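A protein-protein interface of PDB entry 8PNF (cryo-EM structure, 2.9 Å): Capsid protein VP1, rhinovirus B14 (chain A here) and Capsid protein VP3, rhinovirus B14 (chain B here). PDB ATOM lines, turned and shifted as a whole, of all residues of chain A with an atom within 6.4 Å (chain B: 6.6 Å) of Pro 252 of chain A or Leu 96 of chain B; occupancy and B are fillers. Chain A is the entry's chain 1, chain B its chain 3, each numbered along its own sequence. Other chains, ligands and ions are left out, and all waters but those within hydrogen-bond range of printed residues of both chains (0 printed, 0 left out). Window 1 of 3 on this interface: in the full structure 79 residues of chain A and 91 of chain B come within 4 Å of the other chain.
The side-chain amino group (NZ) of Lys 108 of chain A sits close to the backbone carbonyl oxygen (O) of Arg 253 of chain A (3.3 Å).
Hydrophobic or aromatic side chains of chain A that line the printed part of chain B: Pro 252. Of the 17 printed residues of chain B, 2 touch a printed residue of chain A. Along chain B the printed residues that touch a printed residue of chain A span positions 96 to 99. Among the printed residues, 3 pairs touch across the chains.
Pro 252 of chain A touches two residues of chain B. Of chain A, only Pro 252 (3.97 Å) comes within 4 Å of Leu 96 of chain B. Printed residues of chain A within 4 Å of Glu 99 of chain B: Lys 108 (2.5 Å) and Pro 252 (3.6 Å). Printed residues of chain B within 4 Å of Lys 108 of chain A: Glu 99. Val 49 of chain B touches none of the printed residues of chain A. The nearest residue of chain B that does not touch Pro 252 of chain A is Thr 95 of chain B (5.5 Å).
CD1 of Leu 96 of chain B touches CD of Pro 252 of chain A (3.97 Å). OE2 of Glu 99 of chain B touches CB of Pro 252 of chain A (3.6 Å).
The side-chain carboxylate (OE1) of Glu 99 of chain B is in salt-bridge range of the side-chain amino group (NZ) of Lys 108 of chain A (2.5 Å).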
ATOM      1  N   LYS A 108     -12.715  10.921  25.463  1.00  0.00           N
ATOM      2  CA  LYS A 108     -14.036  11.533  25.390  1.00  0.00           C
ATOM      3  C   LYS A 108     -14.200  12.655  26.406  1.00  0.00           C
ATOM      4  O   LYS A 108     -14.849  13.664  26.110  1.00  0.00           O
ATOM      5  CB  LYS A 108     -15.124  10.483  25.587  1.00  0.00           C
ATOM      6  CG  LYS A 108     -16.520  11.026  25.343  1.00  0.00           C
ATOM      7  CD  LYS A 108     -17.597  10.003  25.520  1.00  0.00           C
ATOM      8  CE  LYS A 108     -18.924  10.645  25.233  1.00  0.00           C
ATOM      9  NZ  LYS A 108     -20.046   9.693  25.281  1.00  0.00           N
ATOM     10  N   GLU A 111     -12.245  15.552  24.839  1.00  0.00           N
ATOM     11  CA  GLU A 111     -12.842  16.078  23.622  1.00  0.00           C
ATOM     12  C   GLU A 111     -14.272  16.555  23.815  1.00  0.00           C
ATOM     13  O   GLU A 111     -15.007  16.685  22.833  1.00  0.00           O
ATOM     14  CB  GLU A 111     -12.789  15.029  22.516  1.00  0.00           C
ATOM     15  CG  GLU A 111     -11.399  14.746  22.013  1.00  0.00           C
ATOM     16  CD  GLU A 111     -11.408  13.905  20.761  1.00  0.00           C
ATOM     17  OE1 GLU A 111     -10.333  13.717  20.163  1.00  0.00           O
ATOM     18  OE2 GLU A 111     -12.497  13.441  20.370  1.00  0.00           O
ATOM     19  N   LEU A 112     -14.688  16.806  25.057  1.00  0.00           N
ATOM     20  CA  LEU A 112     -15.848  17.653  25.281  1.00  0.00           C
ATOM     21  C   LEU A 112     -15.519  19.121  25.066  1.00  0.00           C
ATOM     22  O   LEU A 112     -16.434  19.941  25.022  1.00  0.00           O
ATOM     23  CB  LEU A 112     -16.398  17.458  26.691  1.00  0.00           C
ATOM     24  CG  LEU A 112     -17.004  16.104  27.046  1.00  0.00           C
ATOM     25  CD1 LEU A 112     -17.362  16.078  28.511  1.00  0.00           C
ATOM     26  CD2 LEU A 112     -18.226  15.839  26.192  1.00  0.00           C
ATOM     27  N   ARG A 250     -17.893  21.154  23.191  1.00  0.00           N
ATOM     28  CA  ARG A 250     -18.249  20.512  21.937  1.00  0.00           C
ATOM     29  C   ARG A 250     -19.317  19.458  22.171  1.00  0.00           C
ATOM     30  O   ARG A 250     -19.634  19.099  23.305  1.00  0.00           O
ATOM     31  CB  ARG A 250     -17.019  19.885  21.282  1.00  0.00           C
ATOM     32  CG  ARG A 250     -15.865  20.822  21.164  1.00  0.00           C
ATOM     33  CD  ARG A 250     -14.702  20.159  20.501  1.00  0.00           C
ATOM     34  NE  ARG A 250     -14.960  19.805  19.111  1.00  0.00           N
ATOM     35  CZ  ARG A 250     -14.811  20.634  18.087  1.00  0.00           C
ATOM     36  NH1 ARG A 250     -14.410  21.878  18.287  1.00  0.00           N
ATOM     37  NH2 ARG A 250     -15.058  20.220  16.857  1.00  0.00           N
ATOM     38  N   ALA A 251     -19.884  18.980  21.070  1.00  0.00           N
ATOM     39  CA  ALA A 251     -20.806  17.860  21.132  1.00  0.00           C
ATOM     40  C   ALA A 251     -20.055  16.595  21.541  1.00  0.00           C
ATOM     41  O   ALA A 251     -18.930  16.370  21.085  1.00  0.00           O
ATOM     42  CB  ALA A 251     -21.484  17.656  19.784  1.00  0.00           C
ATOM     43  N   PRO A 252     -20.623  15.781  22.428  1.00  0.00           N
ATOM     44  CA  PRO A 252     -19.965  14.527  22.802  1.00  0.00           C
ATOM     45  C   PRO A 252     -19.950  13.537  21.651  1.00  0.00           C
ATOM     46  O   PRO A 252     -20.871  13.479  20.834  1.00  0.00           O
ATOM     47  CB  PRO A 252     -20.818  14.009  23.965  1.00  0.00           C
ATOM     48  CG  PRO A 252     -21.599  15.182  24.427  1.00  0.00           C
ATOM     49  CD  PRO A 252     -21.829  16.027  23.233  1.00  0.00           C
ATOM     50  N   ARG A 253     -18.880  12.755  21.589  1.00  0.00           N
ATOM     51  CA  ARG A 253     -18.774  11.739  20.557  1.00  0.00           C
ATOM     52  C   ARG A 253     -19.468  10.461  20.985  1.00  0.00           C
ATOM     53  O   ARG A 253     -19.269   9.971  22.094  1.00  0.00           O
ATOM     54  CB  ARG A 253     -17.320  11.425  20.238  1.00  0.00           C
ATOM     55  CG  ARG A 253     -17.178  10.870  18.846  1.00  0.00           C
ATOM     56  CD  ARG A 253     -15.847  10.272  18.658  1.00  0.00           C
ATOM     57  NE  ARG A 253     -15.725   9.490  17.444  1.00  0.00           N
ATOM     58  CZ  ARG A 253     -15.161   9.940  16.334  1.00  0.00           C
ATOM     59  NH1 ARG A 253     -14.662  11.163  16.288  1.00  0.00           N
ATOM     60  NH2 ARG A 253     -15.086   9.162  15.276  1.00  0.00           N
ATOM     61  N   ALA A 254     -20.274   9.909  20.087  1.00  0.00           N
ATOM     62  CA  ALA A 254     -20.934   8.645  20.363  1.00  0.00           C
ATOM     63  C   ALA A 254     -20.430   7.511  19.483  1.00  0.00           C
ATOM     64  O   ALA A 254     -20.470   6.348  19.892  1.00  0.00           O
ATOM     65  CB  ALA A 254     -22.442   8.800  20.220  1.00  0.00           C
ATOM     66  N   LEU A 255     -19.983   7.816  18.280  1.00  0.00           N
ATOM     67  CA  LEU A 255     -19.399   6.764  17.469  1.00  0.00           C
ATOM     68  C   LEU A 255     -17.983   6.455  17.951  1.00  0.00           C
ATOM     69  O   LEU A 255     -17.305   7.331  18.490  1.00  0.00           O
ATOM     70  CB  LEU A 255     -19.380   7.176  16.004  1.00  0.00           C
ATOM     71  CG  LEU A 255     -20.767   7.334  15.391  1.00  0.00           C
ATOM     72  CD1 LEU A 255     -20.627   7.768  13.974  1.00  0.00           C
ATOM     73  CD2 LEU A 255     -21.539   6.038  15.478  1.00  0.00           C
ATOM     74  N   ILE B  46     -22.782  23.970  31.157  1.00  0.00           N
ATOM     75  CA  ILE B  46     -23.049  23.600  29.774  1.00  0.00           C
ATOM     76  C   ILE B  46     -24.161  22.566  29.652  1.00  0.00           C
ATOM     77  O   ILE B  46     -24.461  22.126  28.541  1.00  0.00           O
ATOM     78  CB  ILE B  46     -21.775  23.108  29.069  1.00  0.00           C
ATOM     79  CG1 ILE B  46     -21.323  21.768  29.641  1.00  0.00           C
ATOM     80  CG2 ILE B  46     -20.670  24.144  29.183  1.00  0.00           C
ATOM     81  CD1 ILE B  46     -20.317  21.065  28.787  1.00  0.00           C
ATOM     82  N   ILE B  47     -24.782  22.161  30.762  1.00  0.00           N
ATOM     83  CA  ILE B  47     -25.983  21.339  30.676  1.00  0.00           C
ATOM     84  C   ILE B  47     -27.245  22.152  30.860  1.00  0.00           C
ATOM     85  O   ILE B  47     -28.344  21.587  30.856  1.00  0.00           O
ATOM     86  CB  ILE B  47     -25.973  20.170  31.677  1.00  0.00           C
ATOM     87  CG1 ILE B  47     -25.821  20.675  33.104  1.00  0.00           C
ATOM     88  CG2 ILE B  47     -24.910  19.172  31.322  1.00  0.00           C
ATOM     89  CD1 ILE B  47     -26.019  19.594  34.098  1.00  0.00           C
ATOM     90  N   VAL B  49     -27.796  24.287  28.553  1.00  0.00           N
ATOM     91  CA  VAL B  49     -28.006  24.586  27.142  1.00  0.00           C
ATOM     92  C   VAL B  49     -28.892  23.497  26.559  1.00  0.00           C
ATOM     93  O   VAL B  49     -28.636  22.307  26.768  1.00  0.00           O
ATOM     94  CB  VAL B  49     -26.663  24.662  26.395  1.00  0.00           C
ATOM     95  CG1 VAL B  49     -26.855  25.207  25.001  1.00  0.00           C
ATOM     96  CG2 VAL B  49     -25.682  25.519  27.154  1.00  0.00           C
ATOM     97  N   ASP B  50     -29.950  23.901  25.855  1.00  0.00           N
ATOM     98  CA  ASP B  50     -30.826  22.941  25.195  1.00  0.00           C
ATOM     99  C   ASP B  50     -30.106  22.253  24.046  1.00  0.00           C
ATOM    100  O   ASP B  50     -29.395  22.897  23.270  1.00  0.00           O
ATOM    101  CB  ASP B  50     -32.077  23.618  24.641  1.00  0.00           C
ATOM    102  CG  ASP B  50     -33.073  24.000  25.706  1.00  0.00           C
ATOM    103  OD1 ASP B  50     -33.499  23.121  26.484  1.00  0.00           O
ATOM    104  OD2 ASP B  50     -33.501  25.167  25.706  1.00  0.00           O
ATOM    105  N   THR B  51     -30.310  20.947  23.932  1.00  0.00           N
ATOM    106  CA  THR B  51     -29.917  20.175  22.766  1.00  0.00           C
ATOM    107  C   THR B  51     -31.086  19.286  22.376  1.00  0.00           C
ATOM    108  O   THR B  51     -31.929  18.955  23.211  1.00  0.00           O
ATOM    109  CB  THR B  51     -28.665  19.326  23.027  1.00  0.00           C
ATOM    110  OG1 THR B  51     -28.804  18.634  24.270  1.00  0.00           O
ATOM    111  CG2 THR B  51     -27.424  20.196  23.081  1.00  0.00           C
ATOM    112  N   LEU B  52     -31.140  18.917  21.099  1.00  0.00           N
ATOM    113  CA  LEU B  52     -32.281  18.186  20.561  1.00  0.00           C
ATOM    114  C   LEU B  52     -32.349  16.770  21.117  1.00  0.00           C
ATOM    115  O   LEU B  52     -31.321  16.143  21.386  1.00  0.00           O
ATOM    116  CB  LEU B  52     -32.209  18.133  19.038  1.00  0.00           C
ATOM    117  CG  LEU B  52     -32.466  19.451  18.318  1.00  0.00           C
ATOM    118  CD1 LEU B  52     -31.827  19.432  16.947  1.00  0.00           C
ATOM    119  CD2 LEU B  52     -33.949  19.708  18.223  1.00  0.00           C
ATOM    120  N   PHE B  92     -32.996  10.151  25.989  1.00  0.00           N
ATOM    121  CA  PHE B  92     -32.103  11.150  26.555  1.00  0.00           C
ATOM    122  C   PHE B  92     -30.653  10.709  26.579  1.00  0.00           C
ATOM    123  O   PHE B  92     -29.803  11.474  27.035  1.00  0.00           O
ATOM    124  CB  PHE B  92     -32.521  11.494  27.983  1.00  0.00           C
ATOM    125  CG  PHE B  92     -33.891  12.060  28.097  1.00  0.00           C
ATOM    126  CD1 PHE B  92     -34.109  13.416  27.931  1.00  0.00           C
ATOM    127  CD2 PHE B  92     -34.960  11.245  28.417  1.00  0.00           C
ATOM    128  CE1 PHE B  92     -35.376  13.944  28.049  1.00  0.00           C
ATOM    129  CE2 PHE B  92     -36.226  11.764  28.538  1.00  0.00           C
ATOM    130  CZ  PHE B  92     -36.435  13.118  28.351  1.00  0.00           C
ATOM    131  N   LYS B  93     -30.358   9.497  26.111  1.00  0.00           N
ATOM    132  CA  LYS B  93     -29.063   8.881  26.368  1.00  0.00           C
ATOM    133  C   LYS B  93     -27.948   9.534  25.561  1.00  0.00           C
ATOM    134  O   LYS B  93     -26.860   9.779  26.087  1.00  0.00           O
ATOM    135  CB  LYS B  93     -29.152   7.388  26.073  1.00  0.00           C
ATOM    136  CG  LYS B  93     -27.912   6.613  26.411  1.00  0.00           C
ATOM    137  CD  LYS B  93     -28.154   5.126  26.317  1.00  0.00           C
ATOM    138  CE  LYS B  93     -27.072   4.363  27.044  1.00  0.00           C
ATOM    139  NZ  LYS B  93     -27.190   4.545  28.508  1.00  0.00           N
ATOM    140  N   THR B  94     -28.204   9.843  24.294  1.00  0.00           N
ATOM    141  CA  THR B  94     -27.212  10.460  23.425  1.00  0.00           C
ATOM    142  C   THR B  94     -27.231  11.979  23.497  1.00  0.00           C
ATOM    143  O   THR B  94     -26.499  12.634  22.752  1.00  0.00           O
ATOM    144  CB  THR B  94     -27.433  10.017  21.981  1.00  0.00           C
ATOM    145  OG1 THR B  94     -28.798  10.249  21.622  1.00  0.00           O
ATOM    146  CG2 THR B  94     -27.134   8.546  21.836  1.00  0.00           C
ATOM    147  N   THR B  95     -28.053  12.543  24.369  1.00  0.00           N
ATOM    148  CA  THR B  95     -28.230  13.974  24.508  1.00  0.00           C
ATOM    149  C   THR B  95     -27.115  14.530  25.403  1.00  0.00           C
ATOM    150  O   THR B  95     -26.587  13.823  26.265  1.00  0.00           O
ATOM    151  CB  THR B  95     -29.635  14.223  25.075  1.00  0.00           C
ATOM    152  OG1 THR B  95     -30.598  13.669  24.176  1.00  0.00           O
ATOM    153  CG2 THR B  95     -29.960  15.675  25.159  1.00  0.00           C
ATOM    154  N   LEU B  96     -26.735  15.798  25.165  1.00  0.00           N
ATOM    155  CA  LEU B  96     -25.648  16.444  25.902  1.00  0.00           C
ATOM    156  C   LEU B  96     -25.916  16.506  27.402  1.00  0.00           C
ATOM    157  O   LEU B  96     -24.979  16.369  28.201  1.00  0.00           O
ATOM    158  CB  LEU B  96     -25.412  17.850  25.351  1.00  0.00           C
ATOM    159  CG  LEU B  96     -24.561  18.830  26.167  1.00  0.00           C
ATOM    160  CD1 LEU B  96     -23.093  18.469  26.102  1.00  0.00           C
ATOM    161  CD2 LEU B  96     -24.786  20.248  25.719  1.00  0.00           C
ATOM    162  N   LEU B  97     -27.174  16.707  27.801  1.00  0.00           N
ATOM    163  CA  LEU B  97     -27.546  16.493  29.194  1.00  0.00           C
ATOM    164  C   LEU B  97     -27.253  15.059  29.603  1.00  0.00           C
ATOM    165  O   LEU B  97     -26.386  14.815  30.445  1.00  0.00           O
ATOM    166  CB  LEU B  97     -29.023  16.821  29.418  1.00  0.00           C
ATOM    167  CG  LEU B  97     -29.533  16.589  30.849  1.00  0.00           C
ATOM    168  CD1 LEU B  97     -28.880  17.522  31.835  1.00  0.00           C
ATOM    169  CD2 LEU B  97     -31.034  16.715  30.933  1.00  0.00           C
ATOM    170  N   GLY B  98     -27.859  14.102  28.920  1.00  0.00           N
ATOM    171  CA  GLY B  98     -27.727  12.713  29.279  1.00  0.00           C
ATOM    172  C   GLY B  98     -26.455  12.027  28.862  1.00  0.00           C
ATOM    173  O   GLY B  98     -26.375  10.807  28.986  1.00  0.00           O
ATOM    174  N   GLU B  99     -25.466  12.743  28.337  1.00  0.00           N
ATOM    175  CA  GLU B  99     -24.130  12.186  28.183  1.00  0.00           C
ATOM    176  C   GLU B  99     -23.172  12.677  29.255  1.00  0.00           C
ATOM    177  O   GLU B  99     -22.163  12.016  29.514  1.00  0.00           O
ATOM    178  CB  GLU B  99     -23.566  12.502  26.793  1.00  0.00           C
ATOM    179  CG  GLU B  99     -24.193  11.650  25.709  1.00  0.00           C
ATOM    180  CD  GLU B  99     -23.266  11.354  24.557  1.00  0.00           C
ATOM    181  OE1 GLU B  99     -22.231  10.700  24.784  1.00  0.00           O
ATOM    182  OE2 GLU B  99     -23.583  11.761  23.421  1.00  0.00           O
ATOM    183  N   ILE B 100     -23.467  13.817  29.878  1.00  0.00           N
ATOM    184  CA  ILE B 100     -22.771  14.256  31.071  1.00  0.00           C
ATOM    185  C   ILE B 100     -23.400  13.676  32.339  1.00  0.00           C
ATOM    186  O   ILE B 100     -22.681  13.403  33.307  1.00  0.00           O
ATOM    187  CB  ILE B 100     -22.743  15.804  31.096  1.00  0.00           C
ATOM    188  CG1 ILE B 100     -21.798  16.300  30.002  1.00  0.00           C
ATOM    189  CG2 ILE B 100     -22.269  16.400  32.414  1.00  0.00           C
ATOM    190  CD1 ILE B 100     -21.896  17.766  29.710  1.00  0.00           C
ATOM    191  N   VAL B 101     -24.705  13.394  32.315  1.00  0.00           N
ATOM    192  CA  VAL B 101     -25.393  12.707  33.409  1.00  0.00           C
ATOM    193  C   VAL B 101     -24.823  11.308  33.638  1.00  0.00           C
ATOM    194  O   VAL B 101     -24.692  10.859  34.783  1.00  0.00           O
ATOM    195  CB  VAL B 101     -26.911  12.708  33.128  1.00  0.00           C
ATOM    196  CG1 VAL B 101     -27.672  11.835  34.053  1.00  0.00           C
ATOM    197  CG2 VAL B 101     -27.439  14.100  33.377  1.00  0.00           C
ATOM    198  N   ILE B 211     -33.997  19.344  25.695  1.00  0.00           N
ATOM    199  CA  ILE B 211     -33.873  19.177  27.135  1.00  0.00           C
ATOM    200  C   ILE B 211     -32.629  19.922  27.598  1.00  0.00           C
ATOM    201  O   ILE B 211     -31.632  20.031  26.880  1.00  0.00           O
ATOM    202  CB  ILE B 211     -33.867  17.679  27.574  1.00  0.00           C
ATOM    203  CG1 ILE B 211     -34.159  17.509  29.066  1.00  0.00           C
ATOM    204  CG2 ILE B 211     -32.588  16.995  27.272  1.00  0.00           C
ATOM    205  CD1 ILE B 211     -35.578  17.758  29.452  1.00  0.00           C
